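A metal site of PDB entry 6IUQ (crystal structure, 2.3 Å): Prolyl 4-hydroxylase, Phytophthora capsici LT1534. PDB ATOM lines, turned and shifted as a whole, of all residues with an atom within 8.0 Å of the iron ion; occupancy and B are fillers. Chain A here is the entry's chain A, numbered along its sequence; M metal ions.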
ATOM      1  N   LYS A 142     -17.605 -12.794 -24.988  1.00  0.00           N
ATOM      2  CA  LYS A 142     -17.659 -14.228 -25.249  1.00  0.00           C
ATOM      3  C   LYS A 142     -18.187 -14.528 -26.670  1.00  0.00           C
ATOM      4  O   LYS A 142     -19.146 -13.917 -27.128  1.00  0.00           O
ATOM      5  CB  LYS A 142     -18.512 -14.923 -24.190  1.00  0.00           C
ATOM      6  CG  LYS A 142     -18.604 -16.438 -24.324  1.00  0.00           C
ATOM      7  CD  LYS A 142     -19.340 -17.102 -23.145  1.00  0.00           C
ATOM      8  CE  LYS A 142     -20.878 -17.110 -23.329  1.00  0.00           C
ATOM      9  NZ  LYS A 142     -21.381 -17.807 -24.572  1.00  0.00           N
ATOM     10  N   PRO A 154     -31.411 -23.871 -19.790  1.00  0.00           N
ATOM     11  CA  PRO A 154     -32.393 -23.597 -18.749  1.00  0.00           C
ATOM     12  C   PRO A 154     -32.818 -22.127 -18.711  1.00  0.00           C
ATOM     13  O   PRO A 154     -32.124 -21.250 -19.240  1.00  0.00           O
ATOM     14  CB  PRO A 154     -31.669 -24.008 -17.456  1.00  0.00           C
ATOM     15  CG  PRO A 154     -30.236 -24.077 -17.808  1.00  0.00           C
ATOM     16  CD  PRO A 154     -30.138 -24.374 -19.259  1.00  0.00           C
ATOM     17  N   CYS A 155     -33.997 -21.876 -18.129  1.00  0.00           N
ATOM     18  CA  CYS A 155     -34.414 -20.509 -17.817  1.00  0.00           C
ATOM     19  C   CYS A 155     -33.448 -19.936 -16.816  1.00  0.00           C
ATOM     20  O   CYS A 155     -33.097 -20.639 -15.863  1.00  0.00           O
ATOM     21  CB  CYS A 155     -35.823 -20.463 -17.236  1.00  0.00           C
ATOM     22  SG  CYS A 155     -37.115 -20.989 -18.358  1.00  0.00           S
ATOM     23  N   HIS A 156     -33.000 -18.704 -17.005  1.00  0.00           N
ATOM     24  CA  HIS A 156     -32.039 -18.144 -16.060  1.00  0.00           C
ATOM     25  C   HIS A 156     -31.970 -16.634 -16.133  1.00  0.00           C
ATOM     26  O   HIS A 156     -32.466 -16.032 -17.092  1.00  0.00           O
ATOM     27  CB  HIS A 156     -30.614 -18.708 -16.319  1.00  0.00           C
ATOM     28  CG  HIS A 156     -30.077 -18.406 -17.698  1.00  0.00           C
ATOM     29  ND1 HIS A 156     -30.727 -18.795 -18.840  1.00  0.00           N
ATOM     30  CD2 HIS A 156     -29.007 -17.690 -18.113  1.00  0.00           C
ATOM     31  CE1 HIS A 156     -30.042 -18.419 -19.900  1.00  0.00           C
ATOM     32  NE2 HIS A 156     -28.996 -17.717 -19.479  1.00  0.00           N
ATOM     33  N   TYR A 157     -31.322 -16.041 -15.139  1.00  0.00           N
ATOM     34  CA  TYR A 157     -30.861 -14.649 -15.183  1.00  0.00           C
ATOM     35  C   TYR A 157     -29.344 -14.669 -15.439  1.00  0.00           C
ATOM     36  O   TYR A 157     -28.652 -15.521 -14.892  1.00  0.00           O
ATOM     37  CB  TYR A 157     -31.204 -13.924 -13.882  1.00  0.00           C
ATOM     38  CG  TYR A 157     -32.691 -13.755 -13.622  1.00  0.00           C
ATOM     39  CD1 TYR A 157     -33.467 -14.801 -13.134  1.00  0.00           C
ATOM     40  CD2 TYR A 157     -33.314 -12.528 -13.865  1.00  0.00           C
ATOM     41  CE1 TYR A 157     -34.841 -14.623 -12.889  1.00  0.00           C
ATOM     42  CE2 TYR A 157     -34.667 -12.357 -13.624  1.00  0.00           C
ATOM     43  CZ  TYR A 157     -35.426 -13.399 -13.150  1.00  0.00           C
ATOM     44  OH  TYR A 157     -36.770 -13.217 -12.924  1.00  0.00           O
ATOM     45  N   ASP A 158     -28.842 -13.759 -16.266  1.00  0.00           N
ATOM     46  CA  ASP A 158     -27.398 -13.665 -16.545  1.00  0.00           C
ATOM     47  C   ASP A 158     -26.584 -13.348 -15.297  1.00  0.00           C
ATOM     48  O   ASP A 158     -25.434 -13.762 -15.174  1.00  0.00           O
ATOM     49  CB  ASP A 158     -27.137 -12.636 -17.639  1.00  0.00           C
ATOM     50  CG  ASP A 158     -27.260 -13.239 -18.960  1.00  0.00           C
ATOM     51  OD1 ASP A 158     -27.565 -14.446 -18.983  1.00  0.00           O
ATOM     52  OD2 ASP A 158     -27.024 -12.600 -19.979  1.00  0.00           O
ATOM     53  N   ASN A 159     -27.197 -12.615 -14.368  1.00  0.00           N
ATOM     54  CA  ASN A 159     -26.685 -12.438 -13.022  1.00  0.00           C
ATOM     55  C   ASN A 159     -27.699 -13.056 -12.061  1.00  0.00           C
ATOM     56  O   ASN A 159     -28.701 -12.425 -11.742  1.00  0.00           O
ATOM     57  CB  ASN A 159     -26.459 -10.945 -12.708  1.00  0.00           C
ATOM     58  CG  ASN A 159     -25.768 -10.692 -11.382  1.00  0.00           C
ATOM     59  OD1 ASN A 159     -25.800 -11.521 -10.464  1.00  0.00           O
ATOM     60  ND2 ASN A 159     -25.160  -9.513 -11.253  1.00  0.00           N
ATOM     61  N   ARG A 166     -22.376  -8.904 -13.320  1.00  0.00           N
ATOM     62  CA  ARG A 166     -22.999  -8.458 -14.558  1.00  0.00           C
ATOM     63  C   ARG A 166     -24.220  -7.584 -14.339  1.00  0.00           C
ATOM     64  O   ARG A 166     -25.085  -7.892 -13.527  1.00  0.00           O
ATOM     65  CB  ARG A 166     -23.389  -9.654 -15.395  1.00  0.00           C
ATOM     66  CG  ARG A 166     -22.214 -10.440 -15.882  1.00  0.00           C
ATOM     67  CD  ARG A 166     -22.716 -11.818 -16.260  1.00  0.00           C
ATOM     68  NE  ARG A 166     -21.715 -12.660 -16.884  1.00  0.00           N
ATOM     69  CZ  ARG A 166     -21.918 -13.935 -17.218  1.00  0.00           C
ATOM     70  NH1 ARG A 166     -23.109 -14.504 -16.992  1.00  0.00           N
ATOM     71  NH2 ARG A 166     -20.936 -14.618 -17.791  1.00  0.00           N
ATOM     72  N   THR A 169     -26.471  -7.101 -20.342  1.00  0.00           N
ATOM     73  CA  THR A 169     -26.135  -8.118 -21.322  1.00  0.00           C
ATOM     74  C   THR A 169     -26.293  -7.562 -22.726  1.00  0.00           C
ATOM     75  O   THR A 169     -27.310  -6.943 -23.045  1.00  0.00           O
ATOM     76  CB  THR A 169     -27.016  -9.364 -21.175  1.00  0.00           C
ATOM     77  OG1 THR A 169     -26.808  -9.949 -19.874  1.00  0.00           O
ATOM     78  CG2 THR A 169     -26.702 -10.359 -22.286  1.00  0.00           C
ATOM     79  N   LEU A 171     -26.052  -8.743 -26.677  1.00  0.00           N
ATOM     80  CA  LEU A 171     -25.979  -9.857 -27.615  1.00  0.00           C
ATOM     81  C   LEU A 171     -25.926  -9.362 -29.045  1.00  0.00           C
ATOM     82  O   LEU A 171     -26.787  -8.594 -29.473  1.00  0.00           O
ATOM     83  CB  LEU A 171     -27.177 -10.802 -27.406  1.00  0.00           C
ATOM     84  CG  LEU A 171     -27.256 -11.529 -26.055  1.00  0.00           C
ATOM     85  CD1 LEU A 171     -28.601 -12.164 -25.859  1.00  0.00           C
ATOM     86  CD2 LEU A 171     -26.215 -12.608 -25.981  1.00  0.00           C
ATOM     87  N   VAL A 186     -33.952 -16.048 -28.722  1.00  0.00           N
ATOM     88  CA  VAL A 186     -33.901 -15.809 -27.294  1.00  0.00           C
ATOM     89  C   VAL A 186     -35.312 -15.421 -26.902  1.00  0.00           C
ATOM     90  O   VAL A 186     -35.938 -14.593 -27.550  1.00  0.00           O
ATOM     91  CB  VAL A 186     -32.857 -14.732 -26.908  1.00  0.00           C
ATOM     92  CG1 VAL A 186     -33.145 -13.413 -27.593  1.00  0.00           C
ATOM     93  CG2 VAL A 186     -32.800 -14.554 -25.378  1.00  0.00           C
ATOM     94  N   PHE A 208     -30.209  -6.345 -22.592  1.00  0.00           N
ATOM     95  CA  PHE A 208     -31.149  -6.508 -21.506  1.00  0.00           C
ATOM     96  C   PHE A 208     -30.477  -6.478 -20.117  1.00  0.00           C
ATOM     97  O   PHE A 208     -29.255  -6.486 -19.995  1.00  0.00           O
ATOM     98  CB  PHE A 208     -31.994  -7.784 -21.732  1.00  0.00           C
ATOM     99  CG  PHE A 208     -31.224  -9.087 -21.803  1.00  0.00           C
ATOM    100  CD1 PHE A 208     -30.811  -9.735 -20.635  1.00  0.00           C
ATOM    101  CD2 PHE A 208     -31.058  -9.734 -23.012  1.00  0.00           C
ATOM    102  CE1 PHE A 208     -30.160 -10.978 -20.702  1.00  0.00           C
ATOM    103  CE2 PHE A 208     -30.412 -10.982 -23.072  1.00  0.00           C
ATOM    104  CZ  PHE A 208     -29.969 -11.609 -21.896  1.00  0.00           C
ATOM    105  N   SER A 210     -28.998  -7.782 -16.909  1.00  0.00           N
ATOM    106  CA  SER A 210     -28.466  -9.066 -16.472  1.00  0.00           C
ATOM    107  C   SER A 210     -29.109  -9.519 -15.137  1.00  0.00           C
ATOM    108  O   SER A 210     -29.360 -10.719 -14.973  1.00  0.00           O
ATOM    109  CB  SER A 210     -26.949  -8.995 -16.341  1.00  0.00           C
ATOM    110  OG  SER A 210     -26.368  -8.477 -17.554  1.00  0.00           O
ATOM    111  N   MET A 213     -33.742  -9.623 -15.908  1.00  0.00           N
ATOM    112  CA  MET A 213     -34.433 -10.114 -17.085  1.00  0.00           C
ATOM    113  C   MET A 213     -34.318 -11.631 -17.248  1.00  0.00           C
ATOM    114  O   MET A 213     -33.287 -12.157 -17.668  1.00  0.00           O
ATOM    115  CB  MET A 213     -33.911  -9.420 -18.350  1.00  0.00           C
ATOM    116  CG  MET A 213     -34.574  -9.887 -19.618  1.00  0.00           C
ATOM    117  SD  MET A 213     -36.529  -9.671 -19.595  1.00  0.00           S
ATOM    118  CE  MET A 213     -36.649  -7.754 -19.219  1.00  0.00           C
ATOM    119  N   LEU A 214     -35.406 -12.332 -16.920  1.00  0.00           N
ATOM    120  CA  LEU A 214     -35.455 -13.780 -17.074  1.00  0.00           C
ATOM    121  C   LEU A 214     -35.456 -14.123 -18.559  1.00  0.00           C
ATOM    122  O   LEU A 214     -36.122 -13.442 -19.362  1.00  0.00           O
ATOM    123  CB  LEU A 214     -36.696 -14.373 -16.370  1.00  0.00           C
ATOM    124  CG  LEU A 214     -36.851 -15.893 -16.437  1.00  0.00           C
ATOM    125  CD1 LEU A 214     -35.796 -16.598 -15.594  1.00  0.00           C
ATOM    126  CD2 LEU A 214     -38.251 -16.351 -16.044  1.00  0.00           C
ATOM    127  N   HIS A 215     -34.712 -15.144 -18.967  1.00  0.00           N
ATOM    128  CA  HIS A 215     -34.691 -15.533 -20.385  1.00  0.00           C
ATOM    129  C   HIS A 215     -34.227 -16.969 -20.557  1.00  0.00           C
ATOM    130  O   HIS A 215     -33.784 -17.609 -19.622  1.00  0.00           O
ATOM    131  CB  HIS A 215     -33.790 -14.608 -21.208  1.00  0.00           C
ATOM    132  CG  HIS A 215     -32.347 -14.628 -20.795  1.00  0.00           C
ATOM    133  ND1 HIS A 215     -31.893 -13.990 -19.674  1.00  0.00           N
ATOM    134  CD2 HIS A 215     -31.270 -15.224 -21.352  1.00  0.00           C
ATOM    135  CE1 HIS A 215     -30.592 -14.170 -19.556  1.00  0.00           C
ATOM    136  NE2 HIS A 215     -30.188 -14.932 -20.568  1.00  0.00           N
ATOM    137  N   ARG A 216     -34.386 -17.462 -21.778  1.00  0.00           N
ATOM    138  CA  ARG A 216     -33.817 -18.732 -22.182  1.00  0.00           C
ATOM    139  C   ARG A 216     -33.590 -18.650 -23.673  1.00  0.00           C
ATOM    140  O   ARG A 216     -34.144 -17.788 -24.375  1.00  0.00           O
ATOM    141  CB  ARG A 216     -34.756 -19.917 -21.843  1.00  0.00           C
ATOM    142  CG  ARG A 216     -36.051 -19.936 -22.670  1.00  0.00           C
ATOM    143  CD  ARG A 216     -36.988 -21.078 -22.254  1.00  0.00           C
ATOM    144  NE  ARG A 216     -38.339 -20.930 -22.821  1.00  0.00           N
ATOM    145  CZ  ARG A 216     -39.401 -21.660 -22.468  1.00  0.00           C
ATOM    146  NH1 ARG A 216     -39.299 -22.607 -21.531  1.00  0.00           N
ATOM    147  NH2 ARG A 216     -40.567 -21.443 -23.040  1.00  0.00           N
ATOM    148  N   VAL A 217     -32.776 -19.580 -24.165  1.00  0.00           N
ATOM    149  CA  VAL A 217     -32.550 -19.716 -25.592  1.00  0.00           C
ATOM    150  C   VAL A 217     -33.353 -20.922 -26.094  1.00  0.00           C
ATOM    151  O   VAL A 217     -33.334 -21.977 -25.484  1.00  0.00           O
ATOM    152  CB  VAL A 217     -31.041 -19.876 -25.872  1.00  0.00           C
ATOM    153  CG1 VAL A 217     -30.784 -20.182 -27.320  1.00  0.00           C
ATOM    154  CG2 VAL A 217     -30.274 -18.595 -25.453  1.00  0.00           C
ATOM    155  N   THR A 228     -21.329 -12.221 -27.323  1.00  0.00           N
ATOM    156  CA  THR A 228     -21.890 -11.646 -26.102  1.00  0.00           C
ATOM    157  C   THR A 228     -20.920 -10.707 -25.411  1.00  0.00           C
ATOM    158  O   THR A 228     -19.779 -11.042 -25.206  1.00  0.00           O
ATOM    159  CB  THR A 228     -22.281 -12.750 -25.099  1.00  0.00           C
ATOM    160  OG1 THR A 228     -23.123 -13.703 -25.753  1.00  0.00           O
ATOM    161  CG2 THR A 228     -23.016 -12.152 -23.897  1.00  0.00           C
ATOM    162  N   TRP A 230     -20.762  -8.560 -21.784  1.00  0.00           N
ATOM    163  CA  TRP A 230     -21.370  -8.275 -20.499  1.00  0.00           C
ATOM    164  C   TRP A 230     -20.684  -7.087 -19.877  1.00  0.00           C
ATOM    165  O   TRP A 230     -19.462  -7.039 -19.828  1.00  0.00           O
ATOM    166  CB  TRP A 230     -21.284  -9.464 -19.555  1.00  0.00           C
ATOM    167  CG  TRP A 230     -22.331 -10.496 -19.780  1.00  0.00           C
ATOM    168  CD1 TRP A 230     -23.662 -10.389 -19.515  1.00  0.00           C
ATOM    169  CD2 TRP A 230     -22.123 -11.808 -20.284  1.00  0.00           C
ATOM    170  NE1 TRP A 230     -24.317 -11.553 -19.853  1.00  0.00           N
ATOM    171  CE2 TRP A 230     -23.388 -12.449 -20.310  1.00  0.00           C
ATOM    172  CE3 TRP A 230     -20.996 -12.520 -20.720  1.00  0.00           C
ATOM    173  CZ2 TRP A 230     -23.561 -13.765 -20.767  1.00  0.00           C
ATOM    174  CZ3 TRP A 230     -21.169 -13.836 -21.178  1.00  0.00           C
ATOM    175  CH2 TRP A 230     -22.445 -14.440 -21.184  1.00  0.00           C
HETATM  176 FE    FE M   1     -28.121 -15.971 -20.777  1.00  0.00          FE
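OD2 of Asp 158 is in hydrogen-bond range of OG1 of Thr 169, 2.7 Å away.
The backbone carbonyl oxygen (O) of Asp 158 is in hydrogen-bond range of the guanidinium group (NH1) of Arg 166, at 3.0 Å.
The side-chain carboxylate of Asp 158 sits at hydrogen-bond distance from the indole nitrogen of Trp 230 (2.9 Å).
The backbone carbonyl oxygen of Pro 154 lies within hydrogen-bond range of a ring nitrogen (ND1) of His 156, 2.9 Å away.
The backbone NH of Asp 158 lies within hydrogen-bond range of the backbone carbonyl oxygen of Ser 210 (3.3 Å).
A ring nitrogen (ND1) of His 215 sits at hydrogen-bond distance from the backbone carbonyl oxygen (O) of Met 213.
The iron ion is bound by a ring nitrogen (NE2) of His 215 (2.3 Å), a ring nitrogen (NE2) of His 156 (2.3 Å) and the side-chain carboxylate of Asp 158 (2.4 Å).
The iron ion has three donor atoms within binding distance.
Of the 20 residues printed, 3 come within 4 Å of the iron ion.
Along chain A the residues within 4 Å of the iron ion span positions 156 to 215.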
